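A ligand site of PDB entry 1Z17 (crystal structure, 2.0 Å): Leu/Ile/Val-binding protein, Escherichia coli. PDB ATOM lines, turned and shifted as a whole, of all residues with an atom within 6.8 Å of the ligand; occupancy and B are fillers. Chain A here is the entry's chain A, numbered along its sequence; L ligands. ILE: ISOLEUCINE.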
ATOM      1  N   TYR A  18      -2.204  33.724  -1.337  1.00  0.00           N
ATOM      2  CA  TYR A  18      -1.816  33.475  -2.720  1.00  0.00           C
ATOM      3  C   TYR A  18      -0.832  34.553  -3.187  1.00  0.00           C
ATOM      4  O   TYR A  18       0.188  34.235  -3.800  1.00  0.00           O
ATOM      5  CB  TYR A  18      -3.051  33.439  -3.642  1.00  0.00           C
ATOM      6  CG  TYR A  18      -4.063  32.352  -3.298  1.00  0.00           C
ATOM      7  CD1 TYR A  18      -3.660  31.159  -2.675  1.00  0.00           C
ATOM      8  CD2 TYR A  18      -5.412  32.504  -3.617  1.00  0.00           C
ATOM      9  CE1 TYR A  18      -4.589  30.160  -2.381  1.00  0.00           C
ATOM     10  CE2 TYR A  18      -6.341  31.501  -3.337  1.00  0.00           C
ATOM     11  CZ  TYR A  18      -5.930  30.347  -2.721  1.00  0.00           C
ATOM     12  OH  TYR A  18      -6.850  29.366  -2.479  1.00  0.00           O
ATOM     13  N   CYS A  53      -7.854  39.425  -5.523  1.00  0.00           N
ATOM     14  CA  CYS A  53      -8.602  38.304  -6.104  1.00  0.00           C
ATOM     15  C   CYS A  53     -10.086  38.678  -6.155  1.00  0.00           C
ATOM     16  O   CYS A  53     -10.940  37.849  -5.893  1.00  0.00           O
ATOM     17  CB  CYS A  53      -8.426  37.000  -5.310  1.00  0.00           C
ATOM     18  SG  CYS A  53      -7.108  35.954  -6.023  1.00  0.00           S
ATOM     19  N   LEU A  77      -4.076  35.814 -10.235  1.00  0.00           N
ATOM     20  CA  LEU A  77      -4.023  34.500  -9.640  1.00  0.00           C
ATOM     21  C   LEU A  77      -5.365  33.768  -9.718  1.00  0.00           C
ATOM     22  O   LEU A  77      -5.414  32.687 -10.252  1.00  0.00           O
ATOM     23  CB  LEU A  77      -3.565  34.689  -8.183  1.00  0.00           C
ATOM     24  CG  LEU A  77      -2.102  34.749  -7.704  1.00  0.00           C
ATOM     25  CD1 LEU A  77      -1.138  35.034  -8.826  1.00  0.00           C
ATOM     26  CD2 LEU A  77      -1.958  35.768  -6.541  1.00  0.00           C
ATOM     27  N   CYS A  78      -6.429  34.372  -9.162  1.00  0.00           N
ATOM     28  CA  CYS A  78      -7.745  33.729  -9.183  1.00  0.00           C
ATOM     29  C   CYS A  78      -8.350  33.731 -10.576  1.00  0.00           C
ATOM     30  O   CYS A  78      -8.265  34.729 -11.304  1.00  0.00           O
ATOM     31  CB  CYS A  78      -8.675  34.406  -8.174  1.00  0.00           C
ATOM     32  SG  CYS A  78      -8.064  34.185  -6.452  1.00  0.00           S
ATOM     33  N   SER A  79      -8.962  32.610 -10.956  1.00  0.00           N
ATOM     34  CA  SER A  79      -9.550  32.504 -12.290  1.00  0.00           C
ATOM     35  C   SER A  79     -10.589  33.564 -12.588  1.00  0.00           C
ATOM     36  O   SER A  79     -10.574  34.162 -13.669  1.00  0.00           O
ATOM     37  CB  SER A  79     -10.158  31.121 -12.499  1.00  0.00           C
ATOM     38  OG  SER A  79      -9.136  30.135 -12.652  1.00  0.00           O
ATOM     39  N   SER A  80     -11.481  33.835 -11.644  1.00  0.00           N
ATOM     40  CA  SER A  80     -12.551  34.789 -11.926  1.00  0.00           C
ATOM     41  C   SER A  80     -12.051  36.219 -11.996  1.00  0.00           C
ATOM     42  O   SER A  80     -12.773  37.091 -12.474  1.00  0.00           O
ATOM     43  CB  SER A  80     -13.704  34.645 -10.900  1.00  0.00           C
ATOM     44  OG  SER A  80     -13.214  34.832  -9.579  1.00  0.00           O
ATOM     45  N   SER A  81     -10.826  36.460 -11.511  1.00  0.00           N
ATOM     46  CA  SER A  81     -10.202  37.784 -11.576  1.00  0.00           C
ATOM     47  C   SER A  81      -9.304  37.851 -12.829  1.00  0.00           C
ATOM     48  O   SER A  81      -9.213  38.887 -13.518  1.00  0.00           O
ATOM     49  CB  SER A  81      -9.311  38.026 -10.344  1.00  0.00           C
ATOM     50  OG  SER A  81     -10.078  38.303  -9.193  1.00  0.00           O
ATOM     51  N   THR A  82      -8.617  36.759 -13.098  1.00  0.00           N
ATOM     52  CA  THR A  82      -7.715  36.685 -14.236  1.00  0.00           C
ATOM     53  C   THR A  82      -8.418  36.761 -15.588  1.00  0.00           C
ATOM     54  O   THR A  82      -7.915  37.376 -16.526  1.00  0.00           O
ATOM     55  CB  THR A  82      -6.896  35.380 -14.163  1.00  0.00           C
ATOM     56  OG1 THR A  82      -6.059  35.437 -12.992  1.00  0.00           O
ATOM     57  CG2 THR A  82      -6.011  35.225 -15.415  1.00  0.00           C
ATOM     58  N   PRO A  99       0.614  32.592 -13.183  1.00  0.00           N
ATOM     59  CA  PRO A  99       1.303  31.498 -12.493  1.00  0.00           C
ATOM     60  C   PRO A  99       0.325  30.714 -11.603  1.00  0.00           C
ATOM     61  O   PRO A  99       0.742  29.787 -10.893  1.00  0.00           O
ATOM     62  CB  PRO A  99       2.348  32.225 -11.646  1.00  0.00           C
ATOM     63  CG  PRO A  99       1.551  33.445 -11.183  1.00  0.00           C
ATOM     64  CD  PRO A  99       0.822  33.883 -12.470  1.00  0.00           C
ATOM     65  N   ALA A 100      -0.970  31.046 -11.659  1.00  0.00           N
ATOM     66  CA  ALA A 100      -1.921  30.339 -10.797  1.00  0.00           C
ATOM     67  C   ALA A 100      -3.352  30.088 -11.273  1.00  0.00           C
ATOM     68  O   ALA A 100      -4.030  29.216 -10.694  1.00  0.00           O
ATOM     69  CB  ALA A 100      -1.936  31.027  -9.414  1.00  0.00           C
ATOM     70  N   ALA A 101      -3.832  30.819 -12.264  1.00  0.00           N
ATOM     71  CA  ALA A 101      -5.215  30.622 -12.740  1.00  0.00           C
ATOM     72  C   ALA A 101      -5.335  29.295 -13.484  1.00  0.00           C
ATOM     73  O   ALA A 101      -4.623  29.046 -14.469  1.00  0.00           O
ATOM     74  CB  ALA A 101      -5.631  31.744 -13.644  1.00  0.00           C
ATOM     75  N   THR A 102      -6.271  28.453 -13.034  1.00  0.00           N
ATOM     76  CA  THR A 102      -6.430  27.121 -13.632  1.00  0.00           C
ATOM     77  C   THR A 102      -7.696  26.811 -14.435  1.00  0.00           C
ATOM     78  O   THR A 102      -7.765  25.769 -15.093  1.00  0.00           O
ATOM     79  CB  THR A 102      -6.279  26.049 -12.526  1.00  0.00           C
ATOM     80  OG1 THR A 102      -7.222  26.336 -11.481  1.00  0.00           O
ATOM     81  CG2 THR A 102      -4.864  26.089 -11.917  1.00  0.00           C
ATOM     82  N   ALA A 103      -8.701  27.678 -14.377  1.00  0.00           N
ATOM     83  CA  ALA A 103      -9.953  27.434 -15.107  1.00  0.00           C
ATOM     84  C   ALA A 103      -9.639  27.348 -16.609  1.00  0.00           C
ATOM     85  O   ALA A 103      -8.989  28.217 -17.171  1.00  0.00           O
ATOM     86  CB  ALA A 103     -10.957  28.570 -14.841  1.00  0.00           C
ATOM     87  N   ARG A 116       0.224  30.403 -19.335  1.00  0.00           N
ATOM     88  CA  ARG A 116       0.219  29.999 -17.925  1.00  0.00           C
ATOM     89  C   ARG A 116       1.498  29.248 -17.560  1.00  0.00           C
ATOM     90  O   ARG A 116       2.156  28.685 -18.427  1.00  0.00           O
ATOM     91  CB  ARG A 116      -0.936  29.036 -17.606  1.00  0.00           C
ATOM     92  CG  ARG A 116      -2.301  29.344 -18.225  1.00  0.00           C
ATOM     93  CD  ARG A 116      -3.427  28.524 -17.538  1.00  0.00           C
ATOM     94  NE  ARG A 116      -4.563  28.297 -18.431  1.00  0.00           N
ATOM     95  CZ  ARG A 116      -5.850  28.377 -18.071  1.00  0.00           C
ATOM     96  NH1 ARG A 116      -6.806  28.143 -18.972  1.00  0.00           N
ATOM     97  NH2 ARG A 116      -6.182  28.695 -16.819  1.00  0.00           N
ATOM     98  N   THR A 118       1.034  27.251 -14.821  1.00  0.00           N
ATOM     99  CA  THR A 118       0.368  26.273 -13.951  1.00  0.00           C
ATOM    100  C   THR A 118      -0.514  25.439 -14.884  1.00  0.00           C
ATOM    101  O   THR A 118      -0.645  25.773 -16.083  1.00  0.00           O
ATOM    102  CB  THR A 118      -0.517  26.918 -12.844  1.00  0.00           C
ATOM    103  OG1 THR A 118      -0.974  25.871 -11.964  1.00  0.00           O
ATOM    104  CG2 THR A 118      -1.740  27.610 -13.424  1.00  0.00           C
ATOM    105  N   ASP A 121      -7.701  22.856 -14.813  1.00  0.00           N
ATOM    106  CA  ASP A 121      -8.625  22.093 -14.009  1.00  0.00           C
ATOM    107  C   ASP A 121      -9.261  20.979 -14.801  1.00  0.00           C
ATOM    108  O   ASP A 121      -9.882  20.094 -14.221  1.00  0.00           O
ATOM    109  CB  ASP A 121      -9.648  23.016 -13.370  1.00  0.00           C
ATOM    110  CG  ASP A 121      -9.003  23.895 -12.325  1.00  0.00           C
ATOM    111  OD1 ASP A 121      -8.072  23.400 -11.660  1.00  0.00           O
ATOM    112  OD2 ASP A 121      -9.393  25.056 -12.189  1.00  0.00           O
ATOM    113  N   GLN A 124      -6.794  18.742 -13.389  1.00  0.00           N
ATOM    114  CA  GLN A 124      -6.862  18.640 -11.921  1.00  0.00           C
ATOM    115  C   GLN A 124      -8.132  17.929 -11.427  1.00  0.00           C
ATOM    116  O   GLN A 124      -8.058  17.100 -10.527  1.00  0.00           O
ATOM    117  CB  GLN A 124      -6.727  20.015 -11.261  1.00  0.00           C
ATOM    118  CG  GLN A 124      -6.537  19.884  -9.731  1.00  0.00           C
ATOM    119  CD  GLN A 124      -6.145  21.161  -9.009  1.00  0.00           C
ATOM    120  OE1 GLN A 124      -5.666  21.089  -7.876  1.00  0.00           O
ATOM    121  NE2 GLN A 124      -6.359  22.326  -9.618  1.00  0.00           N
ATOM    122  N   GLN A 149     -15.975  30.458 -10.421  1.00  0.00           N
ATOM    123  CA  GLN A 149     -15.500  29.769 -11.615  1.00  0.00           C
ATOM    124  C   GLN A 149     -14.548  28.620 -11.289  1.00  0.00           C
ATOM    125  O   GLN A 149     -14.710  27.516 -11.778  1.00  0.00           O
ATOM    126  CB  GLN A 149     -14.776  30.768 -12.548  1.00  0.00           C
ATOM    127  CG  GLN A 149     -14.363  30.145 -13.888  1.00  0.00           C
ATOM    128  CD  GLN A 149     -13.725  31.140 -14.843  1.00  0.00           C
ATOM    129  OE1 GLN A 149     -13.833  30.994 -16.059  1.00  0.00           O
ATOM    130  NE2 GLN A 149     -13.058  32.152 -14.302  1.00  0.00           N
ATOM    131  N   TYR A 150     -13.559  28.887 -10.461  1.00  0.00           N
ATOM    132  CA  TYR A 150     -12.572  27.880 -10.067  1.00  0.00           C
ATOM    133  C   TYR A 150     -13.194  26.709  -9.314  1.00  0.00           C
ATOM    134  O   TYR A 150     -13.176  25.566  -9.793  1.00  0.00           O
ATOM    135  CB  TYR A 150     -11.496  28.517  -9.168  1.00  0.00           C
ATOM    136  CG  TYR A 150     -10.527  27.519  -8.536  1.00  0.00           C
ATOM    137  CD1 TYR A 150      -9.592  26.839  -9.320  1.00  0.00           C
ATOM    138  CD2 TYR A 150     -10.522  27.286  -7.162  1.00  0.00           C
ATOM    139  CE1 TYR A 150      -8.661  25.952  -8.737  1.00  0.00           C
ATOM    140  CE2 TYR A 150      -9.612  26.402  -6.572  1.00  0.00           C
ATOM    141  CZ  TYR A 150      -8.676  25.751  -7.366  1.00  0.00           C
ATOM    142  OH  TYR A 150      -7.689  24.971  -6.771  1.00  0.00           O
ATOM    143  N   GLY A 151     -13.739  26.994  -8.142  1.00  0.00           N
ATOM    144  CA  GLY A 151     -14.286  25.943  -7.307  1.00  0.00           C
ATOM    145  C   GLY A 151     -15.438  25.177  -7.902  1.00  0.00           C
ATOM    146  O   GLY A 151     -15.485  23.930  -7.840  1.00  0.00           O
ATOM    147  N   LEU A 154     -14.213  22.889 -10.790  1.00  0.00           N
ATOM    148  CA  LEU A 154     -13.586  21.635 -10.318  1.00  0.00           C
ATOM    149  C   LEU A 154     -14.646  20.696  -9.752  1.00  0.00           C
ATOM    150  O   LEU A 154     -14.626  19.475 -10.017  1.00  0.00           O
ATOM    151  CB  LEU A 154     -12.568  21.941  -9.228  1.00  0.00           C
ATOM    152  CG  LEU A 154     -11.218  22.402  -9.784  1.00  0.00           C
ATOM    153  CD1 LEU A 154     -10.407  23.083  -8.697  1.00  0.00           C
ATOM    154  CD2 LEU A 154     -10.491  21.151 -10.345  1.00  0.00           C
ATOM    155  N   GLY A 201     -12.783  24.817  -4.007  1.00  0.00           N
ATOM    156  CA  GLY A 201     -12.711  26.193  -3.546  1.00  0.00           C
ATOM    157  C   GLY A 201     -11.353  26.575  -2.975  1.00  0.00           C
ATOM    158  O   GLY A 201     -10.347  25.937  -3.291  1.00  0.00           O
ATOM    159  N   TYR A 202     -11.355  27.603  -2.121  1.00  0.00           N
ATOM    160  CA  TYR A 202     -10.147  28.138  -1.503  1.00  0.00           C
ATOM    161  C   TYR A 202     -10.040  27.829  -0.012  1.00  0.00           C
ATOM    162  O   TYR A 202     -11.011  27.446   0.621  1.00  0.00           O
ATOM    163  CB  TYR A 202     -10.080  29.657  -1.704  1.00  0.00           C
ATOM    164  CG  TYR A 202     -10.213  30.080  -3.158  1.00  0.00           C
ATOM    165  CD1 TYR A 202      -9.483  29.451  -4.156  1.00  0.00           C
ATOM    166  CD2 TYR A 202     -11.021  31.153  -3.504  1.00  0.00           C
ATOM    167  CE1 TYR A 202      -9.545  29.885  -5.475  1.00  0.00           C
ATOM    168  CE2 TYR A 202     -11.102  31.605  -4.843  1.00  0.00           C
ATOM    169  CZ  TYR A 202     -10.344  30.961  -5.823  1.00  0.00           C
ATOM    170  OH  TYR A 202     -10.339  31.431  -7.122  1.00  0.00           O
ATOM    171  N   GLU A 226      -5.603  22.491  -5.343  1.00  0.00           N
ATOM    172  CA  GLU A 226      -4.435  23.213  -4.853  1.00  0.00           C
ATOM    173  C   GLU A 226      -4.716  24.535  -4.135  1.00  0.00           C
ATOM    174  O   GLU A 226      -3.893  24.999  -3.349  1.00  0.00           O
ATOM    175  CB  GLU A 226      -3.405  23.396  -5.998  1.00  0.00           C
ATOM    176  CG  GLU A 226      -3.268  24.799  -6.560  1.00  0.00           C
ATOM    177  CD  GLU A 226      -4.417  25.222  -7.472  1.00  0.00           C
ATOM    178  OE1 GLU A 226      -4.389  26.371  -7.963  1.00  0.00           O
ATOM    179  OE2 GLU A 226      -5.340  24.394  -7.716  1.00  0.00           O
ATOM    180  N   GLY A 227      -5.883  25.137  -4.373  1.00  0.00           N
ATOM    181  CA  GLY A 227      -6.223  26.379  -3.698  1.00  0.00           C
ATOM    182  C   GLY A 227      -6.392  26.212  -2.186  1.00  0.00           C
ATOM    183  O   GLY A 227      -6.507  27.183  -1.418  1.00  0.00           O
ATOM    184  N   VAL A 228      -6.380  24.955  -1.757  1.00  0.00           N
ATOM    185  CA  VAL A 228      -6.581  24.610  -0.354  1.00  0.00           C
ATOM    186  C   VAL A 228      -5.284  24.075   0.302  1.00  0.00           C
ATOM    187  O   VAL A 228      -5.166  23.955   1.525  1.00  0.00           O
ATOM    188  CB  VAL A 228      -7.731  23.576  -0.334  1.00  0.00           C
ATOM    189  CG1 VAL A 228      -7.415  22.442   0.513  1.00  0.00           C
ATOM    190  CG2 VAL A 228      -9.033  24.260  -0.015  1.00  0.00           C
ATOM    191  N   PHE A 276       2.950  28.532  -5.512  1.00  0.00           N
ATOM    192  CA  PHE A 276       3.006  29.710  -6.375  1.00  0.00           C
ATOM    193  C   PHE A 276       4.310  30.469  -6.295  1.00  0.00           C
ATOM    194  O   PHE A 276       4.566  31.389  -7.075  1.00  0.00           O
ATOM    195  CB  PHE A 276       1.807  30.623  -6.148  1.00  0.00           C
ATOM    196  CG  PHE A 276       0.481  29.887  -6.256  1.00  0.00           C
ATOM    197  CD1 PHE A 276       0.317  28.877  -7.203  1.00  0.00           C
ATOM    198  CD2 PHE A 276      -0.585  30.202  -5.414  1.00  0.00           C
ATOM    199  CE1 PHE A 276      -0.871  28.178  -7.310  1.00  0.00           C
ATOM    200  CE2 PHE A 276      -1.780  29.496  -5.510  1.00  0.00           C
ATOM    201  CZ  PHE A 276      -1.924  28.482  -6.465  1.00  0.00           C
HETATM  202  N   ILE L   1      -6.116  27.974  -9.167  1.00  0.00           N
HETATM  203  CA  ILE L   1      -7.143  28.813  -8.499  1.00  0.00           C
HETATM  204  C   ILE L   1      -7.914  29.746  -9.459  1.00  0.00           C
HETATM  205  O   ILE L   1      -7.694  29.653 -10.698  1.00  0.00           O
HETATM  206  CB  ILE L   1      -6.493  29.653  -7.360  1.00  0.00           C
HETATM  207  CG1 ILE L   1      -5.240  30.337  -7.873  1.00  0.00           C
HETATM  208  CG2 ILE L   1      -6.086  28.755  -6.187  1.00  0.00           C
HETATM  209  CD1 ILE L   1      -4.468  31.063  -6.754  1.00  0.00           C
HETATM  210  OXT ILE L   1      -8.740  30.555  -8.965  1.00  0.00           O
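The side-chain hydroxyl (OG1) of Thr 102 is in hydrogen-bond range of a nitrogen (N) of the ligand (3.0 Å).
A nitrogen (N) of the ligand lies within salt-bridge range of the side-chain carboxylate of Glu 226.
N of the ligand is in hydrogen-bond range of O of Ala 100, at 2.9 Å.
The side-chain hydroxyl (OH) of Tyr 202 is in hydrogen-bond range of an oxygen (OXT) of the ligand (2.6 Å).
The side-chain hydroxyl of Ser 79 sits at hydrogen-bond distance from an oxygen (O) of the ligand (2.5 Å).
The backbone NH (N) of Thr 102 is in hydrogen-bond range of an oxygen (O) of the ligand (3.0 Å).
The backbone NH of Ser 79 is in hydrogen-bond range of an oxygen (OXT) of the ligand (2.9 Å).
Tyr 18 touches the ligand.
Leu 77 touches the ligand (O to CG1, 3.3 Å).
Cys 78 touches the ligand (CA to OXT, 3.3 Å).
CA of Ala 101 touches O of the ligand, at 3.4 Å.
Tyr 150 touches the ligand.
Gly 227 touches the ligand (CA to CG2, 3.4 Å).
Phe 276 touches the ligand (CE2 to CD1, 3.4 Å).
Hydrophobic or aromatic side chains that line the ligand: Tyr 18, Ala 100, Tyr 150, Tyr 202 and Phe 276.
Of the 27 residues printed, 12 come within 4 Å of the ligand.
The side-chain hydroxyl of Thr 82 lies within hydrogen-bond range of the backbone NH of Leu 77.
OG1 of Thr 82 sits at hydrogen-bond distance from O of Cys 78.
The backbone NH of Ala 101 sits at hydrogen-bond distance from the backbone carbonyl oxygen of Leu 77, at 3.2 Å.
OG of Ser 79 lies within hydrogen-bond range of N of Ala 103 (3.0 Å).
The backbone NH (N) of Glu 226 lies within hydrogen-bond range of the side-chain amide oxygen (OE1) of Gln 124 (2.9 Å).
The backbone carbonyl oxygen of Gly 227 is in hydrogen-bond range of the side-chain hydroxyl of Tyr 18 (2.5 Å).
N of Thr 102 sits at hydrogen-bond distance from OG of Ser 79.
The side-chain sulfur of Cys 78 is disulfide-bonded to the side-chain sulfur of Cys 53, at 2.1 Å.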
